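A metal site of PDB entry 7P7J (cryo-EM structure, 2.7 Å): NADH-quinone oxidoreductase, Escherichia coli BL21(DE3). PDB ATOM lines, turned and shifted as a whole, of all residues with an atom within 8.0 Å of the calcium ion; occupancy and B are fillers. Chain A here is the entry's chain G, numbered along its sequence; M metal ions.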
ATOM      1  N   GLU A 614     -20.599 -21.450 -13.216  1.00  0.00           N
ATOM      2  CA  GLU A 614     -20.180 -20.256 -12.495  1.00  0.00           C
ATOM      3  C   GLU A 614     -18.680 -20.019 -12.595  1.00  0.00           C
ATOM      4  O   GLU A 614     -18.129 -19.249 -11.798  1.00  0.00           O
ATOM      5  CB  GLU A 614     -20.609 -20.358 -11.030  1.00  0.00           C
ATOM      6  CG  GLU A 614     -22.087 -20.638 -10.850  1.00  0.00           C
ATOM      7  CD  GLU A 614     -22.345 -21.930 -10.130  1.00  0.00           C
ATOM      8  OE1 GLU A 614     -21.399 -22.733  -9.967  1.00  0.00           O
ATOM      9  OE2 GLU A 614     -23.506 -22.165  -9.728  1.00  0.00           O
ATOM     10  N   SER A 615     -18.012 -20.648 -13.560  1.00  0.00           N
ATOM     11  CA  SER A 615     -16.569 -20.540 -13.654  1.00  0.00           C
ATOM     12  C   SER A 615     -16.148 -20.587 -15.113  1.00  0.00           C
ATOM     13  O   SER A 615     -16.907 -21.014 -15.983  1.00  0.00           O
ATOM     14  CB  SER A 615     -15.869 -21.652 -12.873  1.00  0.00           C
ATOM     15  OG  SER A 615     -16.285 -22.925 -13.314  1.00  0.00           O
ATOM     16  N   ASP A 616     -14.926 -20.137 -15.365  1.00  0.00           N
ATOM     17  CA  ASP A 616     -14.258 -20.281 -16.644  1.00  0.00           C
ATOM     18  C   ASP A 616     -13.161 -21.316 -16.517  1.00  0.00           C
ATOM     19  O   ASP A 616     -12.700 -21.638 -15.426  1.00  0.00           O
ATOM     20  CB  ASP A 616     -13.664 -18.946 -17.116  1.00  0.00           C
ATOM     21  CG  ASP A 616     -14.604 -17.789 -16.893  1.00  0.00           C
ATOM     22  OD1 ASP A 616     -15.589 -17.673 -17.646  1.00  0.00           O
ATOM     23  OD2 ASP A 616     -14.347 -16.998 -15.970  1.00  0.00           O
ATOM     24  N   GLY A 617     -12.724 -21.850 -17.648  1.00  0.00           N
ATOM     25  CA  GLY A 617     -11.632 -22.799 -17.613  1.00  0.00           C
ATOM     26  C   GLY A 617     -11.441 -23.481 -18.949  1.00  0.00           C
ATOM     27  O   GLY A 617     -12.122 -23.184 -19.932  1.00  0.00           O
ATOM     28  N   PHE A 630     -16.858 -20.982 -20.541  1.00  0.00           N
ATOM     29  CA  PHE A 630     -16.992 -19.627 -20.020  1.00  0.00           C
ATOM     30  C   PHE A 630     -18.048 -19.612 -18.928  1.00  0.00           C
ATOM     31  O   PHE A 630     -18.940 -20.450 -18.890  1.00  0.00           O
ATOM     32  CB  PHE A 630     -17.375 -18.647 -21.138  1.00  0.00           C
ATOM     33  CG  PHE A 630     -16.331 -18.505 -22.213  1.00  0.00           C
ATOM     34  CD1 PHE A 630     -16.219 -19.428 -23.231  1.00  0.00           C
ATOM     35  CD2 PHE A 630     -15.470 -17.433 -22.200  1.00  0.00           C
ATOM     36  CE1 PHE A 630     -15.262 -19.289 -24.209  1.00  0.00           C
ATOM     37  CE2 PHE A 630     -14.508 -17.281 -23.175  1.00  0.00           C
ATOM     38  CZ  PHE A 630     -14.400 -18.214 -24.182  1.00  0.00           C
ATOM     39  N   GLN A 631     -17.918 -18.637 -18.027  1.00  0.00           N
ATOM     40  CA  GLN A 631     -18.900 -18.479 -16.953  1.00  0.00           C
ATOM     41  C   GLN A 631     -20.237 -18.016 -17.509  1.00  0.00           C
ATOM     42  O   GLN A 631     -20.294 -17.144 -18.387  1.00  0.00           O
ATOM     43  CB  GLN A 631     -18.371 -17.489 -15.919  1.00  0.00           C
ATOM     44  CG  GLN A 631     -19.272 -17.315 -14.718  1.00  0.00           C
ATOM     45  CD  GLN A 631     -18.694 -16.357 -13.697  1.00  0.00           C
ATOM     46  OE1 GLN A 631     -17.588 -15.856 -13.862  1.00  0.00           O
ATOM     47  NE2 GLN A 631     -19.451 -16.100 -12.639  1.00  0.00           N
ATOM     48  N   VAL A 632     -21.316 -18.599 -17.007  1.00  0.00           N
ATOM     49  CA  VAL A 632     -22.646 -18.231 -17.469  1.00  0.00           C
ATOM     50  C   VAL A 632     -23.209 -17.045 -16.700  1.00  0.00           C
ATOM     51  O   VAL A 632     -23.762 -16.129 -17.291  1.00  0.00           O
ATOM     52  CB  VAL A 632     -23.588 -19.449 -17.369  1.00  0.00           C
ATOM     53  CG1 VAL A 632     -24.866 -19.194 -18.146  1.00  0.00           C
ATOM     54  CG2 VAL A 632     -22.900 -20.687 -17.876  1.00  0.00           C
ATOM     55  N   TYR A 633     -23.044 -17.052 -15.382  1.00  0.00           N
ATOM     56  CA  TYR A 633     -23.656 -16.023 -14.550  1.00  0.00           C
ATOM     57  C   TYR A 633     -22.796 -15.821 -13.311  1.00  0.00           C
ATOM     58  O   TYR A 633     -22.003 -16.685 -12.938  1.00  0.00           O
ATOM     59  CB  TYR A 633     -25.082 -16.394 -14.164  1.00  0.00           C
ATOM     60  CG  TYR A 633     -25.189 -17.545 -13.200  1.00  0.00           C
ATOM     61  CD1 TYR A 633     -25.037 -18.856 -13.630  1.00  0.00           C
ATOM     62  CD2 TYR A 633     -25.469 -17.328 -11.859  1.00  0.00           C
ATOM     63  CE1 TYR A 633     -25.136 -19.905 -12.748  1.00  0.00           C
ATOM     64  CE2 TYR A 633     -25.560 -18.374 -10.971  1.00  0.00           C
ATOM     65  CZ  TYR A 633     -25.395 -19.666 -11.429  1.00  0.00           C
ATOM     66  OH  TYR A 633     -25.503 -20.705 -10.541  1.00  0.00           O
ATOM     67  N   ASP A 634     -22.966 -14.656 -12.693  1.00  0.00           N
ATOM     68  CA  ASP A 634     -22.310 -14.375 -11.423  1.00  0.00           C
ATOM     69  C   ASP A 634     -23.205 -14.833 -10.283  1.00  0.00           C
ATOM     70  O   ASP A 634     -24.348 -14.366 -10.182  1.00  0.00           O
ATOM     71  CB  ASP A 634     -22.019 -12.892 -11.294  1.00  0.00           C
ATOM     72  CG  ASP A 634     -21.098 -12.595 -10.134  1.00  0.00           C
ATOM     73  OD1 ASP A 634     -19.928 -13.012 -10.176  1.00  0.00           O
ATOM     74  OD2 ASP A 634     -21.547 -11.930  -9.177  1.00  0.00           O
ATOM     75  N   PRO A 635     -22.732 -15.737  -9.425  1.00  0.00           N
ATOM     76  CA  PRO A 635     -23.597 -16.230  -8.338  1.00  0.00           C
ATOM     77  C   PRO A 635     -23.899 -15.190  -7.277  1.00  0.00           C
ATOM     78  O   PRO A 635     -24.856 -15.372  -6.515  1.00  0.00           O
ATOM     79  CB  PRO A 635     -22.801 -17.408  -7.748  1.00  0.00           C
ATOM     80  CG  PRO A 635     -21.712 -17.677  -8.727  1.00  0.00           C
ATOM     81  CD  PRO A 635     -21.425 -16.404  -9.424  1.00  0.00           C
ATOM     82  N   LEU A 645     -16.207 -18.715  -5.909  1.00  0.00           N
ATOM     83  CA  LEU A 645     -15.191 -18.314  -6.866  1.00  0.00           C
ATOM     84  C   LEU A 645     -14.716 -19.519  -7.666  1.00  0.00           C
ATOM     85  O   LEU A 645     -15.019 -20.665  -7.360  1.00  0.00           O
ATOM     86  CB  LEU A 645     -14.009 -17.658  -6.148  1.00  0.00           C
ATOM     87  CG  LEU A 645     -14.350 -16.430  -5.309  1.00  0.00           C
ATOM     88  CD1 LEU A 645     -13.230 -16.142  -4.348  1.00  0.00           C
ATOM     89  CD2 LEU A 645     -14.608 -15.245  -6.201  1.00  0.00           C
ATOM     90  N   GLU A 646     -13.956 -19.216  -8.721  1.00  0.00           N
ATOM     91  CA  GLU A 646     -13.283 -20.248  -9.492  1.00  0.00           C
ATOM     92  C   GLU A 646     -12.280 -20.987  -8.614  1.00  0.00           C
ATOM     93  O   GLU A 646     -11.704 -20.426  -7.684  1.00  0.00           O
ATOM     94  CB  GLU A 646     -12.565 -19.637 -10.693  1.00  0.00           C
ATOM     95  CG  GLU A 646     -13.471 -19.185 -11.814  1.00  0.00           C
ATOM     96  CD  GLU A 646     -13.975 -17.769 -11.656  1.00  0.00           C
ATOM     97  OE1 GLU A 646     -13.798 -17.187 -10.568  1.00  0.00           O
ATOM     98  OE2 GLU A 646     -14.546 -17.241 -12.631  1.00  0.00           O
ATOM     99  N   TRP A 648      -9.368 -22.267  -9.572  1.00  0.00           N
ATOM    100  CA  TRP A 648      -8.034 -21.723  -9.814  1.00  0.00           C
ATOM    101  C   TRP A 648      -7.868 -20.365  -9.148  1.00  0.00           C
ATOM    102  O   TRP A 648      -6.764 -20.027  -8.708  1.00  0.00           O
ATOM    103  CB  TRP A 648      -7.742 -21.620 -11.308  1.00  0.00           C
ATOM    104  CG  TRP A 648      -8.802 -20.935 -12.117  1.00  0.00           C
ATOM    105  CD1 TRP A 648      -9.835 -21.528 -12.769  1.00  0.00           C
ATOM    106  CD2 TRP A 648      -8.911 -19.530 -12.375  1.00  0.00           C
ATOM    107  NE1 TRP A 648     -10.592 -20.581 -13.405  1.00  0.00           N
ATOM    108  CE2 TRP A 648     -10.044 -19.348 -13.179  1.00  0.00           C
ATOM    109  CE3 TRP A 648      -8.166 -18.415 -11.996  1.00  0.00           C
ATOM    110  CZ2 TRP A 648     -10.454 -18.088 -13.607  1.00  0.00           C
ATOM    111  CZ3 TRP A 648      -8.571 -17.174 -12.420  1.00  0.00           C
ATOM    112  CH2 TRP A 648      -9.707 -17.014 -13.226  1.00  0.00           C
ATOM    113  N   ARG A 649      -8.944 -19.584  -9.045  1.00  0.00           N
ATOM    114  CA  ARG A 649      -8.879 -18.315  -8.320  1.00  0.00           C
ATOM    115  C   ARG A 649      -8.621 -18.547  -6.828  1.00  0.00           C
ATOM    116  O   ARG A 649      -7.776 -17.878  -6.234  1.00  0.00           O
ATOM    117  CB  ARG A 649     -10.174 -17.530  -8.538  1.00  0.00           C
ATOM    118  CG  ARG A 649     -10.266 -16.249  -7.757  1.00  0.00           C
ATOM    119  CD  ARG A 649     -11.271 -15.301  -8.383  1.00  0.00           C
ATOM    120  NE  ARG A 649     -10.653 -14.460  -9.408  1.00  0.00           N
ATOM    121  CZ  ARG A 649     -11.049 -14.410 -10.677  1.00  0.00           C
ATOM    122  NH1 ARG A 649     -12.059 -15.142 -11.110  1.00  0.00           N
ATOM    123  NH2 ARG A 649     -10.415 -13.610 -11.512  1.00  0.00           N
ATOM    124  N   THR A 666      -6.578 -13.325  -9.202  1.00  0.00           N
ATOM    125  CA  THR A 666      -5.885 -13.091 -10.461  1.00  0.00           C
ATOM    126  C   THR A 666      -6.882 -13.027 -11.615  1.00  0.00           C
ATOM    127  O   THR A 666      -8.098 -12.940 -11.420  1.00  0.00           O
ATOM    128  CB  THR A 666      -4.832 -14.165 -10.684  1.00  0.00           C
ATOM    129  OG1 THR A 666      -4.209 -13.952 -11.960  1.00  0.00           O
ATOM    130  CG2 THR A 666      -5.463 -15.538 -10.659  1.00  0.00           C
ATOM    131  N   LEU A 668      -7.897 -14.857 -15.550  1.00  0.00           N
ATOM    132  CA  LEU A 668      -7.829 -16.171 -16.197  1.00  0.00           C
ATOM    133  C   LEU A 668      -6.637 -16.269 -17.145  1.00  0.00           C
ATOM    134  O   LEU A 668      -5.971 -17.306 -17.201  1.00  0.00           O
ATOM    135  CB  LEU A 668      -9.132 -16.453 -16.944  1.00  0.00           C
ATOM    136  CG  LEU A 668      -9.186 -17.725 -17.800  1.00  0.00           C
ATOM    137  CD1 LEU A 668      -9.111 -18.964 -16.936  1.00  0.00           C
ATOM    138  CD2 LEU A 668     -10.432 -17.752 -18.655  1.00  0.00           C
ATOM    139  N   ARG A 703     -23.727 -11.982 -23.521  1.00  0.00           N
ATOM    140  CA  ARG A 703     -24.201 -13.236 -22.955  1.00  0.00           C
ATOM    141  C   ARG A 703     -25.709 -13.394 -23.025  1.00  0.00           C
ATOM    142  O   ARG A 703     -26.201 -14.523 -23.018  1.00  0.00           O
ATOM    143  CB  ARG A 703     -23.772 -13.363 -21.482  1.00  0.00           C
ATOM    144  CG  ARG A 703     -22.404 -13.961 -21.270  1.00  0.00           C
ATOM    145  CD  ARG A 703     -22.189 -14.240 -19.800  1.00  0.00           C
ATOM    146  NE  ARG A 703     -20.883 -14.823 -19.534  1.00  0.00           N
ATOM    147  CZ  ARG A 703     -19.803 -14.115 -19.212  1.00  0.00           C
ATOM    148  NH1 ARG A 703     -19.843 -12.797 -19.100  1.00  0.00           N
ATOM    149  NH2 ARG A 703     -18.653 -14.748 -18.992  1.00  0.00           N
ATOM    150  N   GLN A 727     -18.978  -7.294 -13.473  1.00  0.00           N
ATOM    151  CA  GLN A 727     -17.877  -7.152 -14.415  1.00  0.00           C
ATOM    152  C   GLN A 727     -17.206  -8.489 -14.658  1.00  0.00           C
ATOM    153  O   GLN A 727     -17.041  -9.292 -13.734  1.00  0.00           O
ATOM    154  CB  GLN A 727     -16.869  -6.129 -13.895  1.00  0.00           C
ATOM    155  CG  GLN A 727     -17.315  -4.699 -14.060  1.00  0.00           C
ATOM    156  CD  GLN A 727     -17.445  -4.300 -15.515  1.00  0.00           C
ATOM    157  OE1 GLN A 727     -18.550  -4.068 -16.005  1.00  0.00           O
ATOM    158  NE2 GLN A 727     -16.321  -4.215 -16.199  1.00  0.00           N
ATOM    159  N   ASP A 728     -16.825  -8.735 -15.908  1.00  0.00           N
ATOM    160  CA  ASP A 728     -16.111  -9.942 -16.294  1.00  0.00           C
ATOM    161  C   ASP A 728     -14.712  -9.542 -16.712  1.00  0.00           C
ATOM    162  O   ASP A 728     -14.501  -9.071 -17.839  1.00  0.00           O
ATOM    163  CB  ASP A 728     -16.835 -10.685 -17.415  1.00  0.00           C
ATOM    164  CG  ASP A 728     -16.358 -12.108 -17.568  1.00  0.00           C
ATOM    165  OD1 ASP A 728     -15.665 -12.607 -16.664  1.00  0.00           O
ATOM    166  OD2 ASP A 728     -16.683 -12.737 -18.595  1.00  0.00           O
ATOM    167  N   ILE A 729     -13.746  -9.728 -15.811  1.00  0.00           N
ATOM    168  CA  ILE A 729     -12.363  -9.464 -16.154  1.00  0.00           C
ATOM    169  C   ILE A 729     -11.665 -10.693 -16.730  1.00  0.00           C
ATOM    170  O   ILE A 729     -10.623 -10.548 -17.376  1.00  0.00           O
ATOM    171  CB  ILE A 729     -11.585  -8.949 -14.927  1.00  0.00           C
ATOM    172  CG1 ILE A 729     -11.470 -10.043 -13.866  1.00  0.00           C
ATOM    173  CG2 ILE A 729     -12.266  -7.727 -14.351  1.00  0.00           C
ATOM    174  CD1 ILE A 729     -10.581  -9.670 -12.706  1.00  0.00           C
ATOM    175  N   ASP A 730     -12.224 -11.886 -16.534  1.00  0.00           N
ATOM    176  CA  ASP A 730     -11.559 -13.105 -16.971  1.00  0.00           C
ATOM    177  C   ASP A 730     -11.677 -13.322 -18.469  1.00  0.00           C
ATOM    178  O   ASP A 730     -10.712 -13.756 -19.114  1.00  0.00           O
ATOM    179  CB  ASP A 730     -12.128 -14.306 -16.226  1.00  0.00           C
ATOM    180  CG  ASP A 730     -11.856 -14.250 -14.736  1.00  0.00           C
ATOM    181  OD1 ASP A 730     -10.736 -13.855 -14.346  1.00  0.00           O
ATOM    182  OD2 ASP A 730     -12.756 -14.603 -13.954  1.00  0.00           O
ATOM    183  N   THR A 731     -12.841 -13.049 -19.043  1.00  0.00           N
ATOM    184  CA  THR A 731     -13.131 -13.424 -20.422  1.00  0.00           C
ATOM    185  C   THR A 731     -13.579 -12.220 -21.234  1.00  0.00           C
ATOM    186  O   THR A 731     -13.766 -11.112 -20.718  1.00  0.00           O
ATOM    187  CB  THR A 731     -14.203 -14.512 -20.498  1.00  0.00           C
ATOM    188  OG1 THR A 731     -15.455 -13.982 -20.051  1.00  0.00           O
ATOM    189  CG2 THR A 731     -13.830 -15.700 -19.616  1.00  0.00           C
ATOM    190  N   PHE A 735     -21.629  -9.702 -18.870  1.00  0.00           N
ATOM    191  CA  PHE A 735     -22.853 -10.166 -18.214  1.00  0.00           C
ATOM    192  C   PHE A 735     -24.018  -9.223 -18.495  1.00  0.00           C
ATOM    193  O   PHE A 735     -24.687  -8.722 -17.596  1.00  0.00           O
ATOM    194  CB  PHE A 735     -22.619 -10.318 -16.716  1.00  0.00           C
ATOM    195  CG  PHE A 735     -21.702 -11.436 -16.348  1.00  0.00           C
ATOM    196  CD1 PHE A 735     -22.134 -12.745 -16.372  1.00  0.00           C
ATOM    197  CD2 PHE A 735     -20.386 -11.174 -15.984  1.00  0.00           C
ATOM    198  CE1 PHE A 735     -21.284 -13.780 -16.031  1.00  0.00           C
ATOM    199  CE2 PHE A 735     -19.538 -12.199 -15.645  1.00  0.00           C
ATOM    200  CZ  PHE A 735     -19.987 -13.502 -15.669  1.00  0.00           C
HETATM  201 CA    CA M   1     -15.127 -15.378 -14.178  1.00  0.00          CA
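The guanidinium group (NH1) of Arg 649 lies within salt-bridge range of the side-chain carboxylate (OE1) of Glu 646.
OD1 of Asp 730 lies within salt-bridge range of NH2 of Arg 649 (2.9 Å).
The backbone NH of Leu 668 sits at hydrogen-bond distance from the side-chain carboxylate of Asp 730, at 3.2 Å.
The backbone NH of Gln 631 sits at hydrogen-bond distance from the backbone carbonyl oxygen of Ser 615 (3.3 Å).
O of Gln 631 lies within hydrogen-bond range of NE of Arg 703, 2.7 Å away.
NE2 of Gln 631 sits at hydrogen-bond distance from O of Tyr 633, at 2.6 Å.
The backbone carbonyl oxygen of Asp 616 sits at hydrogen-bond distance from the indole nitrogen of Trp 648 (3.1 Å).
OD2 of Asp 728 lies within salt-bridge range of NH2 of Arg 703 (2.8 Å).
The calcium ion is bound by OE2 of Glu 646 (2.5 Å), OD2 of Asp 730 (2.5 Å), OE1 of Gln 631 (2.5 Å) and OD2 of Asp 616 (2.5 Å).
Merely in contact with the calcium ion: Asp 728.
Five residues have an atom within 4 Å of the calcium ion: Asp 616, Gln 631, Glu 646, Asp 728 and Asp 730.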
